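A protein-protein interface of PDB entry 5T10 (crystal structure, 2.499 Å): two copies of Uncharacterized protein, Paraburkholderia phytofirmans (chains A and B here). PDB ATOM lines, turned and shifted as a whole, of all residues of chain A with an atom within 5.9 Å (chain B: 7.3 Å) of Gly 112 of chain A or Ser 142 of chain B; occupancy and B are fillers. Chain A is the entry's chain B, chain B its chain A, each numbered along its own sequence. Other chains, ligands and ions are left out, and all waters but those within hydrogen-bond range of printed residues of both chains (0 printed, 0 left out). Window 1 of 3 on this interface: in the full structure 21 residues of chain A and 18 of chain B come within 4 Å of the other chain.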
ATOM      1  N   ALA A  95     -26.789  -4.183 -19.342  1.00  0.00           N
ATOM      2  CA  ALA A  95     -25.609  -3.782 -18.605  1.00  0.00           C
ATOM      3  C   ALA A  95     -24.365  -4.252 -19.343  1.00  0.00           C
ATOM      4  O   ALA A  95     -24.412  -5.174 -20.158  1.00  0.00           O
ATOM      5  CB  ALA A  95     -25.639  -4.341 -17.197  1.00  0.00           C
ATOM      6  N   VAL A  96     -23.247  -3.607 -19.052  1.00  0.00           N
ATOM      7  CA  VAL A  96     -21.977  -4.041 -19.596  1.00  0.00           C
ATOM      8  C   VAL A  96     -21.154  -4.639 -18.482  1.00  0.00           C
ATOM      9  O   VAL A  96     -20.891  -3.983 -17.473  1.00  0.00           O
ATOM     10  CB  VAL A  96     -21.230  -2.881 -20.260  1.00  0.00           C
ATOM     11  CG1 VAL A  96     -19.871  -3.352 -20.765  1.00  0.00           C
ATOM     12  CG2 VAL A  96     -22.081  -2.321 -21.399  1.00  0.00           C
ATOM     13  N   GLU A  97     -20.765  -5.895 -18.658  1.00  0.00           N
ATOM     14  CA  GLU A  97     -20.020  -6.609 -17.626  1.00  0.00           C
ATOM     15  C   GLU A  97     -18.520  -6.516 -17.857  1.00  0.00           C
ATOM     16  O   GLU A  97     -17.739  -6.609 -16.926  1.00  0.00           O
ATOM     17  CB  GLU A  97     -20.458  -8.075 -17.534  1.00  0.00           C
ATOM     18  CG  GLU A  97     -21.878  -8.274 -17.025  1.00  0.00           C
ATOM     19  CD  GLU A  97     -22.921  -8.166 -18.134  1.00  0.00           C
ATOM     20  OE1 GLU A  97     -22.662  -8.626 -19.274  1.00  0.00           O
ATOM     21  OE2 GLU A  97     -24.009  -7.615 -17.862  1.00  0.00           O
ATOM     22  N   GLU A  98     -18.126  -6.332 -19.108  1.00  0.00           N
ATOM     23  CA  GLU A  98     -16.725  -6.187 -19.459  1.00  0.00           C
ATOM     24  C   GLU A  98     -16.615  -5.383 -20.733  1.00  0.00           C
ATOM     25  O   GLU A  98     -17.397  -5.566 -21.687  1.00  0.00           O
ATOM     26  CB  GLU A  98     -16.079  -7.556 -19.647  1.00  0.00           C
ATOM     27  CG  GLU A  98     -14.579  -7.526 -19.884  1.00  0.00           C
ATOM     28  CD  GLU A  98     -13.916  -8.849 -19.515  1.00  0.00           C
ATOM     29  OE1 GLU A  98     -14.469  -9.917 -19.868  1.00  0.00           O
ATOM     30  OE2 GLU A  98     -12.852  -8.819 -18.845  1.00  0.00           O
ATOM     31  N   TRP A  99     -15.632  -4.494 -20.748  1.00  0.00           N
ATOM     32  CA  TRP A  99     -15.420  -3.584 -21.865  1.00  0.00           C
ATOM     33  C   TRP A  99     -14.028  -3.001 -21.671  1.00  0.00           C
ATOM     34  O   TRP A  99     -13.877  -1.970 -21.023  1.00  0.00           O
ATOM     35  CB  TRP A  99     -16.504  -2.489 -21.840  1.00  0.00           C
ATOM     36  CG  TRP A  99     -16.601  -1.601 -23.050  1.00  0.00           C
ATOM     37  CD1 TRP A  99     -15.687  -0.659 -23.462  1.00  0.00           C
ATOM     38  CD2 TRP A  99     -17.701  -1.525 -23.978  1.00  0.00           C
ATOM     39  NE1 TRP A  99     -16.144  -0.027 -24.591  1.00  0.00           N
ATOM     40  CE2 TRP A  99     -17.371  -0.535 -24.932  1.00  0.00           C
ATOM     41  CE3 TRP A  99     -18.924  -2.203 -24.100  1.00  0.00           C
ATOM     42  CZ2 TRP A  99     -18.222  -0.211 -26.000  1.00  0.00           C
ATOM     43  CZ3 TRP A  99     -19.764  -1.877 -25.148  1.00  0.00           C
ATOM     44  CH2 TRP A  99     -19.407  -0.889 -26.091  1.00  0.00           C
ATOM     45  N   VAL A 110     -11.920  -7.276 -24.841  1.00  0.00           N
ATOM     46  CA  VAL A 110     -12.912  -8.196 -24.307  1.00  0.00           C
ATOM     47  C   VAL A 110     -14.183  -7.426 -24.003  1.00  0.00           C
ATOM     48  O   VAL A 110     -14.142  -6.380 -23.355  1.00  0.00           O
ATOM     49  CB  VAL A 110     -12.392  -8.970 -23.056  1.00  0.00           C
ATOM     50  CG1 VAL A 110     -11.440 -10.056 -23.485  1.00  0.00           C
ATOM     51  CG2 VAL A 110     -11.683  -8.035 -22.059  1.00  0.00           C
ATOM     52  N   VAL A 111     -15.307  -7.928 -24.515  1.00  0.00           N
ATOM     53  CA  VAL A 111     -16.596  -7.296 -24.274  1.00  0.00           C
ATOM     54  C   VAL A 111     -17.514  -8.304 -23.629  1.00  0.00           C
ATOM     55  O   VAL A 111     -17.442  -9.498 -23.933  1.00  0.00           O
ATOM     56  CB  VAL A 111     -17.264  -6.794 -25.591  1.00  0.00           C
ATOM     57  CG1 VAL A 111     -18.525  -6.021 -25.274  1.00  0.00           C
ATOM     58  CG2 VAL A 111     -16.315  -5.906 -26.375  1.00  0.00           C
ATOM     59  N   GLY A 112     -18.375  -7.834 -22.733  1.00  0.00           N
ATOM     60  CA  GLY A 112     -19.392  -8.691 -22.146  1.00  0.00           C
ATOM     61  C   GLY A 112     -20.624  -7.863 -21.891  1.00  0.00           C
ATOM     62  O   GLY A 112     -20.555  -6.856 -21.180  1.00  0.00           O
ATOM     63  N   VAL A 113     -21.746  -8.263 -22.490  1.00  0.00           N
ATOM     64  CA  VAL A 113     -22.980  -7.488 -22.383  1.00  0.00           C
ATOM     65  C   VAL A 113     -24.186  -8.370 -22.111  1.00  0.00           C
ATOM     66  O   VAL A 113     -24.243  -9.519 -22.559  1.00  0.00           O
ATOM     67  CB  VAL A 113     -23.246  -6.608 -23.665  1.00  0.00           C
ATOM     68  CG1 VAL A 113     -22.311  -5.404 -23.715  1.00  0.00           C
ATOM     69  CG2 VAL A 113     -23.086  -7.412 -24.925  1.00  0.00           C
ATOM     70  N   THR A 114     -25.134  -7.837 -21.345  1.00  0.00           N
ATOM     71  CA  THR A 114     -26.463  -8.416 -21.273  1.00  0.00           C
ATOM     72  C   THR A 114     -27.507  -7.397 -21.743  1.00  0.00           C
ATOM     73  O   THR A 114     -27.315  -6.184 -21.602  1.00  0.00           O
ATOM     74  CB  THR A 114     -26.816  -8.883 -19.860  1.00  0.00           C
ATOM     75  OG1 THR A 114     -26.663  -7.793 -18.949  1.00  0.00           O
ATOM     76  CG2 THR A 114     -25.923 -10.046 -19.440  1.00  0.00           C
ATOM     77  N   GLY A 131     -24.038 -11.844 -24.300  1.00  0.00           N
ATOM     78  CA  GLY A 131     -22.994 -12.071 -25.265  1.00  0.00           C
ATOM     79  C   GLY A 131     -21.671 -11.632 -24.692  1.00  0.00           C
ATOM     80  O   GLY A 131     -21.563 -10.578 -24.062  1.00  0.00           O
ATOM     81  N   THR A 132     -20.661 -12.458 -24.902  1.00  0.00           N
ATOM     82  CA  THR A 132     -19.317 -12.076 -24.560  1.00  0.00           C
ATOM     83  C   THR A 132     -18.462 -12.363 -25.766  1.00  0.00           C
ATOM     84  O   THR A 132     -18.820 -13.206 -26.596  1.00  0.00           O
ATOM     85  CB  THR A 132     -18.760 -12.894 -23.371  1.00  0.00           C
ATOM     86  OG1 THR A 132     -18.602 -14.258 -23.771  1.00  0.00           O
ATOM     87  CG2 THR A 132     -19.678 -12.800 -22.159  1.00  0.00           C
ATOM     88  N   ARG A 133     -17.330 -11.669 -25.848  1.00  0.00           N
ATOM     89  CA  ARG A 133     -16.394 -11.855 -26.940  1.00  0.00           C
ATOM     90  C   ARG A 133     -15.007 -11.332 -26.571  1.00  0.00           C
ATOM     91  O   ARG A 133     -14.858 -10.232 -26.030  1.00  0.00           O
ATOM     92  CB  ARG A 133     -16.901 -11.173 -28.210  1.00  0.00           C
ATOM     93  CG  ARG A 133     -16.012 -11.395 -29.436  1.00  0.00           C
ATOM     94  CD  ARG A 133     -16.655 -10.873 -30.721  1.00  0.00           C
ATOM     95  NE  ARG A 133     -17.994 -11.418 -30.909  1.00  0.00           N
ATOM     96  CZ  ARG A 133     -18.735 -11.230 -31.996  1.00  0.00           C
ATOM     97  NH1 ARG A 133     -18.269 -10.512 -33.009  1.00  0.00           N
ATOM     98  NH2 ARG A 133     -19.942 -11.764 -32.069  1.00  0.00           N
ATOM     99  N   LEU A 148     -20.229  -7.540 -31.639  1.00  0.00           N
ATOM    100  CA  LEU A 148     -20.941  -8.366 -30.670  1.00  0.00           C
ATOM    101  C   LEU A 148     -22.337  -7.826 -30.415  1.00  0.00           C
ATOM    102  O   LEU A 148     -23.301  -8.593 -30.394  1.00  0.00           O
ATOM    103  CB  LEU A 148     -20.182  -8.451 -29.342  1.00  0.00           C
ATOM    104  CG  LEU A 148     -20.891  -9.279 -28.248  1.00  0.00           C
ATOM    105  CD1 LEU A 148     -20.835 -10.754 -28.573  1.00  0.00           C
ATOM    106  CD2 LEU A 148     -20.288  -9.017 -26.863  1.00  0.00           C
ATOM    107  N   ILE B  42     -26.196 -11.616 -15.177  1.00  0.00           N
ATOM    108  CA  ILE B  42     -25.969 -12.841 -15.934  1.00  0.00           C
ATOM    109  C   ILE B  42     -26.916 -13.939 -15.456  1.00  0.00           C
ATOM    110  O   ILE B  42     -27.437 -14.714 -16.256  1.00  0.00           O
ATOM    111  CB  ILE B  42     -24.508 -13.283 -15.865  1.00  0.00           C
ATOM    112  CG1 ILE B  42     -23.661 -12.312 -16.659  1.00  0.00           C
ATOM    113  CG2 ILE B  42     -24.309 -14.660 -16.460  1.00  0.00           C
ATOM    114  CD1 ILE B  42     -22.227 -12.171 -16.147  1.00  0.00           C
ATOM    115  N   TRP B  99     -13.572 -13.199  -8.919  1.00  0.00           N
ATOM    116  CA  TRP B  99     -14.040 -12.609 -10.158  1.00  0.00           C
ATOM    117  C   TRP B  99     -12.947 -11.683 -10.660  1.00  0.00           C
ATOM    118  O   TRP B  99     -12.971 -10.482 -10.403  1.00  0.00           O
ATOM    119  CB  TRP B  99     -15.344 -11.849  -9.903  1.00  0.00           C
ATOM    120  CG  TRP B  99     -16.087 -11.358 -11.134  1.00  0.00           C
ATOM    121  CD1 TRP B  99     -15.738 -10.302 -11.934  1.00  0.00           C
ATOM    122  CD2 TRP B  99     -17.318 -11.874 -11.671  1.00  0.00           C
ATOM    123  NE1 TRP B  99     -16.667 -10.142 -12.933  1.00  0.00           N
ATOM    124  CE2 TRP B  99     -17.646 -11.093 -12.794  1.00  0.00           C
ATOM    125  CE3 TRP B  99     -18.173 -12.916 -11.310  1.00  0.00           C
ATOM    126  CZ2 TRP B  99     -18.792 -11.324 -13.564  1.00  0.00           C
ATOM    127  CZ3 TRP B  99     -19.317 -13.142 -12.082  1.00  0.00           C
ATOM    128  CH2 TRP B  99     -19.612 -12.344 -13.187  1.00  0.00           C
ATOM    129  N   TYR B 101      -8.971 -11.450 -13.280  1.00  0.00           N
ATOM    130  CA  TYR B 101      -7.874 -12.031 -14.036  1.00  0.00           C
ATOM    131  C   TYR B 101      -6.778 -12.322 -13.037  1.00  0.00           C
ATOM    132  O   TYR B 101      -6.557 -11.552 -12.106  1.00  0.00           O
ATOM    133  CB  TYR B 101      -7.356 -11.067 -15.133  1.00  0.00           C
ATOM    134  CG  TYR B 101      -8.322 -10.926 -16.274  1.00  0.00           C
ATOM    135  CD1 TYR B 101      -8.528 -11.971 -17.160  1.00  0.00           C
ATOM    136  CD2 TYR B 101      -9.066  -9.763 -16.444  1.00  0.00           C
ATOM    137  CE1 TYR B 101      -9.438 -11.861 -18.185  1.00  0.00           C
ATOM    138  CE2 TYR B 101      -9.972  -9.642 -17.467  1.00  0.00           C
ATOM    139  CZ  TYR B 101     -10.155 -10.691 -18.339  1.00  0.00           C
ATOM    140  OH  TYR B 101     -11.059 -10.583 -19.366  1.00  0.00           O
ATOM    141  N   PRO B 109      -8.496 -15.836 -16.318  1.00  0.00           N
ATOM    142  CA  PRO B 109      -9.687 -15.388 -15.597  1.00  0.00           C
ATOM    143  C   PRO B 109     -10.181 -16.424 -14.579  1.00  0.00           C
ATOM    144  O   PRO B 109     -10.291 -17.618 -14.878  1.00  0.00           O
ATOM    145  CB  PRO B 109     -10.714 -15.182 -16.722  1.00  0.00           C
ATOM    146  CG  PRO B 109     -10.279 -16.109 -17.803  1.00  0.00           C
ATOM    147  CD  PRO B 109      -8.769 -16.105 -17.738  1.00  0.00           C
ATOM    148  N   VAL B 111     -13.278 -17.292 -11.786  1.00  0.00           N
ATOM    149  CA  VAL B 111     -14.585 -17.030 -11.192  1.00  0.00           C
ATOM    150  C   VAL B 111     -14.919 -18.041 -10.091  1.00  0.00           C
ATOM    151  O   VAL B 111     -14.655 -19.241 -10.231  1.00  0.00           O
ATOM    152  CB  VAL B 111     -15.714 -17.082 -12.252  1.00  0.00           C
ATOM    153  CG1 VAL B 111     -17.044 -16.703 -11.626  1.00  0.00           C
ATOM    154  CG2 VAL B 111     -15.397 -16.159 -13.418  1.00  0.00           C
ATOM    155  N   SER B 139      -8.793 -16.256 -22.682  1.00  0.00           N
ATOM    156  CA  SER B 139     -10.236 -16.240 -22.460  1.00  0.00           C
ATOM    157  C   SER B 139     -10.657 -14.939 -21.787  1.00  0.00           C
ATOM    158  O   SER B 139      -9.927 -14.402 -20.954  1.00  0.00           O
ATOM    159  CB  SER B 139     -10.653 -17.425 -21.580  1.00  0.00           C
ATOM    160  OG  SER B 139     -10.220 -18.662 -22.121  1.00  0.00           O
ATOM    161  N   GLY B 140     -11.833 -14.434 -22.141  1.00  0.00           N
ATOM    162  CA  GLY B 140     -12.395 -13.294 -21.441  1.00  0.00           C
ATOM    163  C   GLY B 140     -12.971 -13.681 -20.085  1.00  0.00           C
ATOM    164  O   GLY B 140     -13.502 -14.780 -19.910  1.00  0.00           O
ATOM    165  N   LEU B 141     -12.862 -12.782 -19.111  1.00  0.00           N
ATOM    166  CA  LEU B 141     -13.445 -13.022 -17.793  1.00  0.00           C
ATOM    167  C   LEU B 141     -14.960 -13.120 -17.875  1.00  0.00           C
ATOM    168  O   LEU B 141     -15.567 -13.987 -17.240  1.00  0.00           O
ATOM    169  CB  LEU B 141     -13.065 -11.908 -16.823  1.00  0.00           C
ATOM    170  CG  LEU B 141     -13.670 -12.014 -15.425  1.00  0.00           C
ATOM    171  CD1 LEU B 141     -13.144 -13.242 -14.701  1.00  0.00           C
ATOM    172  CD2 LEU B 141     -13.377 -10.753 -14.638  1.00  0.00           C
ATOM    173  N   SER B 142     -15.567 -12.232 -18.664  1.00  0.00           N
ATOM    174  CA  SER B 142     -17.029 -12.226 -18.847  1.00  0.00           C
ATOM    175  C   SER B 142     -17.548 -13.533 -19.442  1.00  0.00           C
ATOM    176  O   SER B 142     -18.644 -13.962 -19.128  1.00  0.00           O
ATOM    177  CB  SER B 142     -17.482 -11.021 -19.686  1.00  0.00           C
ATOM    178  OG  SER B 142     -16.830 -10.992 -20.945  1.00  0.00           O
ATOM    179  N   SER B 143     -16.738 -14.168 -20.282  1.00  0.00           N
ATOM    180  CA  SER B 143     -17.070 -15.460 -20.864  1.00  0.00           C
ATOM    181  C   SER B 143     -17.067 -16.564 -19.810  1.00  0.00           C
ATOM    182  O   SER B 143     -18.015 -17.338 -19.701  1.00  0.00           O
ATOM    183  CB  SER B 143     -16.046 -15.808 -21.931  1.00  0.00           C
ATOM    184  OG  SER B 143     -15.604 -14.636 -22.584  1.00  0.00           O
ATOM    185  N   VAL B 144     -15.985 -16.637 -19.044  1.00  0.00           N
ATOM    186  CA  VAL B 144     -15.853 -17.650 -18.005  1.00  0.00           C
ATOM    187  C   VAL B 144     -17.031 -17.586 -17.044  1.00  0.00           C
ATOM    188  O   VAL B 144     -17.800 -18.541 -16.930  1.00  0.00           O
ATOM    189  CB  VAL B 144     -14.527 -17.500 -17.241  1.00  0.00           C
ATOM    190  CG1 VAL B 144     -14.532 -18.382 -16.014  1.00  0.00           C
ATOM    191  CG2 VAL B 144     -13.386 -17.875 -18.147  1.00  0.00           C
ATOM    192  N   ALA B 145     -17.185 -16.439 -16.396  1.00  0.00           N
ATOM    193  CA  ALA B 145     -18.329 -16.172 -15.537  1.00  0.00           C
ATOM    194  C   ALA B 145     -19.678 -16.558 -16.162  1.00  0.00           C
ATOM    195  O   ALA B 145     -20.482 -17.257 -15.534  1.00  0.00           O
ATOM    196  CB  ALA B 145     -18.331 -14.710 -15.135  1.00  0.00           C
ATOM    197  N   THR B 146     -19.930 -16.110 -17.390  1.00  0.00           N
ATOM    198  CA  THR B 146     -21.215 -16.396 -18.054  1.00  0.00           C
ATOM    199  C   THR B 146     -21.406 -17.879 -18.265  1.00  0.00           C
ATOM    200  O   THR B 146     -22.472 -18.416 -18.013  1.00  0.00           O
ATOM    201  CB  THR B 146     -21.319 -15.718 -19.429  1.00  0.00           C
ATOM    202  OG1 THR B 146     -21.506 -14.320 -19.236  1.00  0.00           O
ATOM    203  CG2 THR B 146     -22.514 -16.258 -20.208  1.00  0.00           C
ATOM    204  N   SER B 147     -20.353 -18.532 -18.739  1.00  0.00           N
ATOM    205  CA  SER B 147     -20.386 -19.960 -18.989  1.00  0.00           C
ATOM    206  C   SER B 147     -20.584 -20.734 -17.677  1.00  0.00           C
ATOM    207  O   SER B 147     -21.450 -21.600 -17.592  1.00  0.00           O
ATOM    208  CB  SER B 147     -19.103 -20.385 -19.701  1.00  0.00           C
ATOM    209  OG  SER B 147     -19.093 -21.774 -19.961  1.00  0.00           O
ATOM    210  N   LEU B 148     -19.796 -20.391 -16.656  1.00  0.00           N
ATOM    211  CA  LEU B 148     -19.899 -21.016 -15.335  1.00  0.00           C
ATOM    212  C   LEU B 148     -21.295 -20.837 -14.738  1.00  0.00           C
ATOM    213  O   LEU B 148     -21.934 -21.812 -14.353  1.00  0.00           O
ATOM    214  CB  LEU B 148     -18.844 -20.449 -14.377  1.00  0.00           C
ATOM    215  CG  LEU B 148     -18.882 -21.044 -12.961  1.00  0.00           C
ATOM    216  CD1 LEU B 148     -18.622 -22.542 -13.002  1.00  0.00           C
ATOM    217  CD2 LEU B 148     -17.881 -20.366 -12.017  1.00  0.00           C
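Printed residues of chain B within 4 Å of Glu 98 of chain A: Tyr 101, Leu 141 and Ser 142. Printed residues of chain B within 4 Å of Val 110 of chain A: Tyr 101 and Gly 140. Of the printed residues of chain B, Val 111 of chain A touches Ser 142. Gly 112 of chain A touches just one residue of chain B: Ser 142 (3.6 Å). Trp 99 of chain B touches none of the printed residues of chain A. Of chain A, only Glu 98, Val 111, Gly 112 and Thr 132 come within 4 Å of Ser 142 of chain B. Printed residues of chain A within 4 Å of Ser 143 of chain B: Thr 132. Of the printed residues of chain A, Thr 146 of chain B touches Thr 132. The nearest residue of chain B that does not touch Gly 112 of chain A is Ser 143 of chain B (6.4 Å). The nearest residue of chain A that does not touch Ser 142 of chain B is Glu 97 of chain A (4.7 Å).
Among the printed residues, 10 pairs touch across the chains.
Tyr 101 of chain B touches Val 110 of chain A. Val 110 of chain A touches Gly 140 of chain B (CG1 to CA, 3.9 Å). Gly 112 of chain A touches Ser 142 of chain B (CA to OG, 3.6 Å). Thr 132 of chain A touches Ser 142 of chain B. Thr 132 of chain A touches Thr 146 of chain B.
The backbone NH of Leu 141 of chain B sits at hydrogen-bond distance from the side-chain hydroxyl of Tyr 101 of chain B. O of Gly 140 of chain B is in hydrogen-bond range of OG of Ser 143 of chain B (3.4 Å). O of Ser 142 of chain B lies within hydrogen-bond range of OG1 of Thr 146 of chain B. N of Glu 97 of chain A is in hydrogen-bond range of O of Gly 112 of chain A, at 2.7 Å. The backbone carbonyl oxygen of Glu 98 of chain A sits at hydrogen-bond distance from the backbone NH of Gly 112 of chain A (2.7 Å). The backbone carbonyl oxygen of Arg 133 of chain A sits at hydrogen-bond distance from the backbone NH of Val 111 of chain A, 2.8 Å away.
The side-chain hydroxyl (OH) of Tyr 101 of chain B sits at hydrogen-bond distance from the side-chain carboxylate (OE2) of Glu 98 of chain A (2.6 Å). N of Leu 141 of chain B sits at hydrogen-bond distance from OE1 of Glu 98 of chain A, at 3.4 Å. OE1 of Glu 98 of chain A lies within hydrogen-bond range of OG of Ser 142 of chain B. O of Val 111 of chain A lies within hydrogen-bond range of OG of Ser 142 of chain B, 3.4 Å away. The side-chain hydroxyl of Thr 132 of chain A is in hydrogen-bond range of the side-chain hydroxyl of Ser 143 of chain B, 3.2 Å away.
Positions printed for both chains: 99, 111 and 148. Of the 10 pairs that touch across the chains among the printed residues, none has its exchanged pair printed and touching as well.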
